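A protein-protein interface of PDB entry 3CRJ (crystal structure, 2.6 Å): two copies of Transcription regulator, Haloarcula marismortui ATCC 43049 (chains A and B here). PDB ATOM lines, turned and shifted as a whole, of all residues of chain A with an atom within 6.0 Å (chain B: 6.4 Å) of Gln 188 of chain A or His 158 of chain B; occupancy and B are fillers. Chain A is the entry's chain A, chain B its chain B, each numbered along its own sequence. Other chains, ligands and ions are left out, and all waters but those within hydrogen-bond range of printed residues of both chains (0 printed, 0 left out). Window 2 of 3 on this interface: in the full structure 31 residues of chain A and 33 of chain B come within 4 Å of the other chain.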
ATOM      1  N   LEU A 183      -5.968  -3.997 -11.631  1.00  0.00           N
ATOM      2  CA  LEU A 183      -5.295  -5.199 -11.232  1.00  0.00           C
ATOM      3  C   LEU A 183      -6.327  -6.243 -10.839  1.00  0.00           C
ATOM      4  O   LEU A 183      -6.128  -7.440 -11.072  1.00  0.00           O
ATOM      5  CB  LEU A 183      -4.332  -4.914 -10.070  1.00  0.00           C
ATOM      6  CG  LEU A 183      -3.345  -3.749 -10.205  1.00  0.00           C
ATOM      7  CD1 LEU A 183      -2.786  -3.341  -8.841  1.00  0.00           C
ATOM      8  CD2 LEU A 183      -2.235  -4.093 -11.158  1.00  0.00           C
ATOM      9  N   GLU A 184      -7.424  -5.802 -10.237  1.00  0.00           N
ATOM     10  CA  GLU A 184      -8.411  -6.738  -9.730  1.00  0.00           C
ATOM     11  C   GLU A 184      -9.116  -7.402 -10.923  1.00  0.00           C
ATOM     12  O   GLU A 184      -9.325  -8.628 -10.917  1.00  0.00           O
ATOM     13  CB  GLU A 184      -9.377  -6.061  -8.758  1.00  0.00           C
ATOM     14  CG  GLU A 184     -10.439  -6.959  -8.115  1.00  0.00           C
ATOM     15  CD  GLU A 184      -9.865  -8.025  -7.137  1.00  0.00           C
ATOM     16  OE1 GLU A 184      -9.428  -9.125  -7.592  1.00  0.00           O
ATOM     17  OE2 GLU A 184      -9.891  -7.767  -5.897  1.00  0.00           O
ATOM     18  N   THR A 185      -9.416  -6.628 -11.968  1.00  0.00           N
ATOM     19  CA  THR A 185      -9.970  -7.233 -13.185  1.00  0.00           C
ATOM     20  C   THR A 185      -8.930  -8.119 -13.887  1.00  0.00           C
ATOM     21  O   THR A 185      -9.270  -9.225 -14.374  1.00  0.00           O
ATOM     22  CB  THR A 185     -10.538  -6.223 -14.211  1.00  0.00           C
ATOM     23  OG1 THR A 185      -9.478  -5.782 -15.057  1.00  0.00           O
ATOM     24  CG2 THR A 185     -11.241  -5.013 -13.552  1.00  0.00           C
ATOM     25  N   ALA A 186      -7.683  -7.651 -13.952  1.00  0.00           N
ATOM     26  CA  ALA A 186      -6.601  -8.462 -14.538  1.00  0.00           C
ATOM     27  C   ALA A 186      -6.371  -9.782 -13.805  1.00  0.00           C
ATOM     28  O   ALA A 186      -6.067 -10.797 -14.426  1.00  0.00           O
ATOM     29  CB  ALA A 186      -5.304  -7.683 -14.635  1.00  0.00           C
ATOM     30  N   ARG A 187      -6.534  -9.769 -12.488  1.00  0.00           N
ATOM     31  CA  ARG A 187      -6.476 -10.995 -11.719  1.00  0.00           C
ATOM     32  C   ARG A 187      -7.479 -11.978 -12.269  1.00  0.00           C
ATOM     33  O   ARG A 187      -7.150 -13.159 -12.408  1.00  0.00           O
ATOM     34  CB  ARG A 187      -6.732 -10.729 -10.221  1.00  0.00           C
ATOM     35  CG  ARG A 187      -6.503 -11.929  -9.321  1.00  0.00           C
ATOM     36  CD  ARG A 187      -5.181 -12.668  -9.687  1.00  0.00           C
ATOM     37  NE  ARG A 187      -5.034 -13.964  -9.007  1.00  0.00           N
ATOM     38  CZ  ARG A 187      -5.465 -15.132  -9.482  1.00  0.00           C
ATOM     39  NH1 ARG A 187      -6.092 -15.198 -10.658  1.00  0.00           N
ATOM     40  NH2 ARG A 187      -5.278 -16.244  -8.775  1.00  0.00           N
ATOM     41  N   GLN A 188      -8.684 -11.507 -12.595  1.00  0.00           N
ATOM     42  CA  GLN A 188      -9.752 -12.364 -13.143  1.00  0.00           C
ATOM     43  C   GLN A 188      -9.446 -12.824 -14.565  1.00  0.00           C
ATOM     44  O   GLN A 188      -9.685 -14.002 -14.926  1.00  0.00           O
ATOM     45  CB  GLN A 188     -11.100 -11.658 -13.145  1.00  0.00           C
ATOM     46  CG  GLN A 188     -12.205 -12.614 -13.569  1.00  0.00           C
ATOM     47  CD  GLN A 188     -13.593 -11.998 -13.547  1.00  0.00           C
ATOM     48  OE1 GLN A 188     -13.942 -11.282 -12.615  1.00  0.00           O
ATOM     49  NE2 GLN A 188     -14.388 -12.279 -14.574  1.00  0.00           N
ATOM     50  N   THR A 189      -8.923 -11.891 -15.372  1.00  0.00           N
ATOM     51  CA  THR A 189      -8.426 -12.232 -16.697  1.00  0.00           C
ATOM     52  C   THR A 189      -7.383 -13.353 -16.587  1.00  0.00           C
ATOM     53  O   THR A 189      -7.527 -14.410 -17.234  1.00  0.00           O
ATOM     54  CB  THR A 189      -7.825 -11.016 -17.360  1.00  0.00           C
ATOM     55  OG1 THR A 189      -8.826 -10.003 -17.455  1.00  0.00           O
ATOM     56  CG2 THR A 189      -7.309 -11.351 -18.752  1.00  0.00           C
ATOM     57  N   ALA A 190      -6.372 -13.158 -15.739  1.00  0.00           N
ATOM     58  CA  ALA A 190      -5.399 -14.210 -15.480  1.00  0.00           C
ATOM     59  C   ALA A 190      -6.041 -15.564 -15.127  1.00  0.00           C
ATOM     60  O   ALA A 190      -5.640 -16.572 -15.679  1.00  0.00           O
ATOM     61  CB  ALA A 190      -4.404 -13.789 -14.405  1.00  0.00           C
ATOM     62  N   SER A 191      -7.027 -15.618 -14.233  1.00  0.00           N
ATOM     63  CA  SER A 191      -7.647 -16.924 -13.960  1.00  0.00           C
ATOM     64  C   SER A 191      -8.395 -17.488 -15.158  1.00  0.00           C
ATOM     65  O   SER A 191      -8.194 -18.641 -15.515  1.00  0.00           O
ATOM     66  CB  SER A 191      -8.551 -16.932 -12.720  1.00  0.00           C
ATOM     67  OG  SER A 191      -7.806 -17.473 -11.640  1.00  0.00           O
ATOM     68  N   GLU A 192      -9.232 -16.671 -15.795  1.00  0.00           N
ATOM     69  CA  GLU A 192      -9.954 -17.120 -16.976  1.00  0.00           C
ATOM     70  C   GLU A 192      -8.977 -17.639 -18.015  1.00  0.00           C
ATOM     71  O   GLU A 192      -9.153 -18.749 -18.547  1.00  0.00           O
ATOM     72  CB  GLU A 192     -10.818 -15.998 -17.555  1.00  0.00           C
ATOM     73  CG  GLU A 192     -12.037 -15.670 -16.739  1.00  0.00           C
ATOM     74  CD  GLU A 192     -12.587 -14.289 -17.022  1.00  0.00           C
ATOM     75  OE1 GLU A 192     -11.875 -13.454 -17.610  1.00  0.00           O
ATOM     76  OE2 GLU A 192     -13.740 -14.016 -16.636  1.00  0.00           O
ATOM     77  N   TYR A 193      -7.922 -16.868 -18.272  1.00  0.00           N
ATOM     78  CA  TYR A 193      -6.969 -17.257 -19.293  1.00  0.00           C
ATOM     79  C   TYR A 193      -6.355 -18.595 -18.965  1.00  0.00           C
ATOM     80  O   TYR A 193      -6.281 -19.484 -19.831  1.00  0.00           O
ATOM     81  CB  TYR A 193      -5.844 -16.241 -19.488  1.00  0.00           C
ATOM     82  CG  TYR A 193      -4.877 -16.749 -20.521  1.00  0.00           C
ATOM     83  CD1 TYR A 193      -5.235 -16.785 -21.870  1.00  0.00           C
ATOM     84  CD2 TYR A 193      -3.640 -17.257 -20.150  1.00  0.00           C
ATOM     85  CE1 TYR A 193      -4.384 -17.277 -22.814  1.00  0.00           C
ATOM     86  CE2 TYR A 193      -2.771 -17.776 -21.089  1.00  0.00           C
ATOM     87  CZ  TYR A 193      -3.151 -17.785 -22.422  1.00  0.00           C
ATOM     88  OH  TYR A 193      -2.300 -18.309 -23.366  1.00  0.00           O
ATOM     89  N   ASP B 155     -20.031 -11.365 -20.119  1.00  0.00           N
ATOM     90  CA  ASP B 155     -19.857 -10.026 -19.583  1.00  0.00           C
ATOM     91  C   ASP B 155     -18.932  -9.244 -20.544  1.00  0.00           C
ATOM     92  O   ASP B 155     -17.690  -9.323 -20.478  1.00  0.00           O
ATOM     93  CB  ASP B 155     -19.333 -10.039 -18.151  1.00  0.00           C
ATOM     94  CG  ASP B 155     -19.117  -8.642 -17.592  1.00  0.00           C
ATOM     95  OD1 ASP B 155     -19.457  -7.615 -18.240  1.00  0.00           O
ATOM     96  OD2 ASP B 155     -18.596  -8.572 -16.474  1.00  0.00           O
ATOM     97  N   ALA B 156     -19.584  -8.510 -21.442  1.00  0.00           N
ATOM     98  CA  ALA B 156     -18.951  -7.859 -22.561  1.00  0.00           C
ATOM     99  C   ALA B 156     -18.040  -6.755 -22.081  1.00  0.00           C
ATOM    100  O   ALA B 156     -17.039  -6.450 -22.723  1.00  0.00           O
ATOM    101  CB  ALA B 156     -19.999  -7.332 -23.506  1.00  0.00           C
ATOM    102  N   GLU B 157     -18.362  -6.198 -20.923  1.00  0.00           N
ATOM    103  CA  GLU B 157     -17.559  -5.130 -20.344  1.00  0.00           C
ATOM    104  C   GLU B 157     -16.225  -5.696 -19.849  1.00  0.00           C
ATOM    105  O   GLU B 157     -15.160  -5.134 -20.128  1.00  0.00           O
ATOM    106  CB  GLU B 157     -18.333  -4.402 -19.230  1.00  0.00           C
ATOM    107  CG  GLU B 157     -17.654  -3.152 -18.656  1.00  0.00           C
ATOM    108  CD  GLU B 157     -17.627  -1.945 -19.633  1.00  0.00           C
ATOM    109  OE1 GLU B 157     -16.793  -1.025 -19.417  1.00  0.00           O
ATOM    110  OE2 GLU B 157     -18.445  -1.890 -20.600  1.00  0.00           O
ATOM    111  N   HIS B 158     -16.295  -6.818 -19.132  1.00  0.00           N
ATOM    112  CA  HIS B 158     -15.101  -7.504 -18.674  1.00  0.00           C
ATOM    113  C   HIS B 158     -14.304  -8.094 -19.828  1.00  0.00           C
ATOM    114  O   HIS B 158     -13.106  -7.882 -19.923  1.00  0.00           O
ATOM    115  CB  HIS B 158     -15.402  -8.591 -17.654  1.00  0.00           C
ATOM    116  CG  HIS B 158     -14.190  -9.386 -17.279  1.00  0.00           C
ATOM    117  ND1 HIS B 158     -13.287  -8.961 -16.329  1.00  0.00           N
ATOM    118  CD2 HIS B 158     -13.695 -10.548 -17.769  1.00  0.00           C
ATOM    119  CE1 HIS B 158     -12.297  -9.835 -16.236  1.00  0.00           C
ATOM    120  NE2 HIS B 158     -12.523 -10.811 -17.094  1.00  0.00           N
ATOM    121  N   VAL B 159     -14.950  -8.836 -20.721  1.00  0.00           N
ATOM    122  CA  VAL B 159     -14.194  -9.406 -21.838  1.00  0.00           C
ATOM    123  C   VAL B 159     -13.482  -8.297 -22.595  1.00  0.00           C
ATOM    124  O   VAL B 159     -12.328  -8.430 -22.936  1.00  0.00           O
ATOM    125  CB  VAL B 159     -15.050 -10.254 -22.764  1.00  0.00           C
ATOM    126  CG1 VAL B 159     -14.213 -10.716 -23.970  1.00  0.00           C
ATOM    127  CG2 VAL B 159     -15.638 -11.442 -21.979  1.00  0.00           C
ATOM    128  N   THR B 160     -14.161  -7.187 -22.824  1.00  0.00           N
ATOM    129  CA  THR B 160     -13.520  -6.066 -23.475  1.00  0.00           C
ATOM    130  C   THR B 160     -12.323  -5.527 -22.720  1.00  0.00           C
ATOM    131  O   THR B 160     -11.246  -5.388 -23.291  1.00  0.00           O
ATOM    132  CB  THR B 160     -14.497  -4.957 -23.733  1.00  0.00           C
ATOM    133  OG1 THR B 160     -15.367  -5.378 -24.794  1.00  0.00           O
ATOM    134  CG2 THR B 160     -13.759  -3.683 -24.136  1.00  0.00           C
ATOM    135  N   ARG B 161     -12.470  -5.236 -21.437  1.00  0.00           N
ATOM    136  CA  ARG B 161     -11.308  -4.689 -20.764  1.00  0.00           C
ATOM    137  C   ARG B 161     -10.178  -5.707 -20.565  1.00  0.00           C
ATOM    138  O   ARG B 161      -8.998  -5.327 -20.500  1.00  0.00           O
ATOM    139  CB  ARG B 161     -11.667  -3.938 -19.490  1.00  0.00           C
ATOM    140  CG  ARG B 161     -12.308  -4.763 -18.416  1.00  0.00           C
ATOM    141  CD  ARG B 161     -12.541  -3.935 -17.140  1.00  0.00           C
ATOM    142  NE  ARG B 161     -13.075  -2.582 -17.384  1.00  0.00           N
ATOM    143  CZ  ARG B 161     -12.338  -1.461 -17.403  1.00  0.00           C
ATOM    144  NH1 ARG B 161     -11.006  -1.496 -17.214  1.00  0.00           N
ATOM    145  NH2 ARG B 161     -12.943  -0.290 -17.621  1.00  0.00           N
ATOM    146  N   SER B 162     -10.538  -6.983 -20.499  1.00  0.00           N
ATOM    147  CA  SER B 162      -9.569  -8.050 -20.549  1.00  0.00           C
ATOM    148  C   SER B 162      -8.721  -7.944 -21.823  1.00  0.00           C
ATOM    149  O   SER B 162      -7.487  -8.042 -21.752  1.00  0.00           O
ATOM    150  CB  SER B 162     -10.258  -9.415 -20.500  1.00  0.00           C
ATOM    151  OG  SER B 162     -10.666  -9.742 -19.195  1.00  0.00           O
ATOM    152  N   LEU B 163      -9.366  -7.734 -22.976  1.00  0.00           N
ATOM    153  CA  LEU B 163      -8.608  -7.565 -24.214  1.00  0.00           C
ATOM    154  C   LEU B 163      -7.690  -6.341 -24.157  1.00  0.00           C
ATOM    155  O   LEU B 163      -6.574  -6.388 -24.698  1.00  0.00           O
ATOM    156  CB  LEU B 163      -9.508  -7.491 -25.424  1.00  0.00           C
ATOM    157  CG  LEU B 163     -10.254  -8.786 -25.799  1.00  0.00           C
ATOM    158  CD1 LEU B 163     -11.424  -8.458 -26.725  1.00  0.00           C
ATOM    159  CD2 LEU B 163      -9.342  -9.893 -26.372  1.00  0.00           C
ATOM    160  N   TYR B 193      -7.771 -15.891 -25.695  1.00  0.00           N
ATOM    161  CA  TYR B 193      -8.703 -15.420 -24.670  1.00  0.00           C
ATOM    162  C   TYR B 193     -10.111 -15.218 -25.219  1.00  0.00           C
ATOM    163  O   TYR B 193     -11.064 -15.796 -24.723  1.00  0.00           O
ATOM    164  CB  TYR B 193      -8.208 -14.132 -23.989  1.00  0.00           C
ATOM    165  CG  TYR B 193      -9.196 -13.634 -22.957  1.00  0.00           C
ATOM    166  CD1 TYR B 193      -9.376 -14.318 -21.735  1.00  0.00           C
ATOM    167  CD2 TYR B 193      -9.992 -12.523 -23.206  1.00  0.00           C
ATOM    168  CE1 TYR B 193     -10.310 -13.886 -20.785  1.00  0.00           C
ATOM    169  CE2 TYR B 193     -10.937 -12.090 -22.264  1.00  0.00           C
ATOM    170  CZ  TYR B 193     -11.089 -12.771 -21.061  1.00  0.00           C
ATOM    171  OH  TYR B 193     -12.015 -12.322 -20.143  1.00  0.00           O
ATOM    172  N   MET B 197     -13.667 -17.136 -24.265  1.00  0.00           N
ATOM    173  CA  MET B 197     -14.787 -16.477 -23.649  1.00  0.00           C
ATOM    174  C   MET B 197     -16.019 -16.514 -24.550  1.00  0.00           C
ATOM    175  O   MET B 197     -17.108 -16.881 -24.108  1.00  0.00           O
ATOM    176  CB  MET B 197     -14.443 -15.019 -23.364  1.00  0.00           C
ATOM    177  CG  MET B 197     -13.420 -14.795 -22.272  1.00  0.00           C
ATOM    178  SD  MET B 197     -13.553 -15.936 -20.683  1.00  0.00           S
ATOM    179  CE  MET B 197     -12.154 -17.227 -21.069  1.00  0.00           C
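OG1 of Thr 189 of chain A is in hydrogen-bond range of O of Thr 185 of chain A, 3.2 Å away.
The side-chain hydroxyl (OH) of Tyr 193 of chain B is in hydrogen-bond range of the side-chain hydroxyl (OG) of Ser 162 of chain B, at 3.1 Å.
NE2 of His 158 of chain B lies close to OH of Tyr 193 of chain B, at 3.4 Å.
A ring nitrogen (NE2) of His 158 of chain B sits at hydrogen-bond distance from the side-chain hydroxyl (OG) of Ser 162 of chain B (3.0 Å).
The backbone NH (N) of His 158 of chain B sits at hydrogen-bond distance from the side-chain carboxylate (OD1) of Asp 155 of chain B (3.4 Å).
The side-chain amide nitrogen (NE2) of Gln 188 of chain A sits at hydrogen-bond distance from the side-chain carboxylate (OE2) of Glu 192 of chain A (2.8 Å).
Printed residues of chain B within 4 Å of Glu 192 of chain A: His 158 (2.8 Å), Tyr 193 (2.8 Å) and Met 197 (3.96 Å).
Printed residues of chain A within 4 Å of His 158 of chain B: Thr 185 (3.6 Å), Gln 188 (3.5 Å), Thr 189 (3.7 Å) and Glu 192 (2.8 Å).
Of the printed residues of chain A, Arg 161 of chain B touches Thr 185.
Of the printed residues of chain A, Tyr 193 of chain B touches Glu 192.
Printed residues of chain A within 4 Å of Met 197 of chain B: Glu 192.
The nearest residue of chain B that does not touch Gln 188 of chain A is Ser 162 of chain B (5.7 Å).
The nearest residue of chain A that does not touch His 158 of chain B is Ala 186 of chain A (5.6 Å).
The nearest printed residue of chain B that does not touch Thr 185 of chain A is Ser 162 of chain B (5.0 Å).
OE1 of Glu 192 of chain A lies within hydrogen-bond range of NE2 of His 158 of chain B (2.8 Å).
NE2 of His 158 of chain B sits at hydrogen-bond distance from NE2 of Gln 188 of chain A, 3.5 Å away.
The side-chain carboxylate of Glu 192 of chain A sits at hydrogen-bond distance from the side-chain hydroxyl of Tyr 193 of chain B (2.8 Å).
OG1 of Thr 189 of chain A is in hydrogen-bond range of OG of Ser 162 of chain B, 2.5 Å away.
Position printed for both chains: 193.
Of the 8 pairs that touch across the chains among the printed residues, none has its exchanged pair printed and touching as well.
Among the printed residues, pairs that only touch across the chains: Thr 185 of chain A with His 158 of chain B (3.6 Å), Thr 185 of chain A with Arg 161 of chain B (3.97 Å), Thr 189 of chain A with His 158 of chain B (3.7 Å) and Glu 192 of chain A with Met 197 of chain B (3.96 Å).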
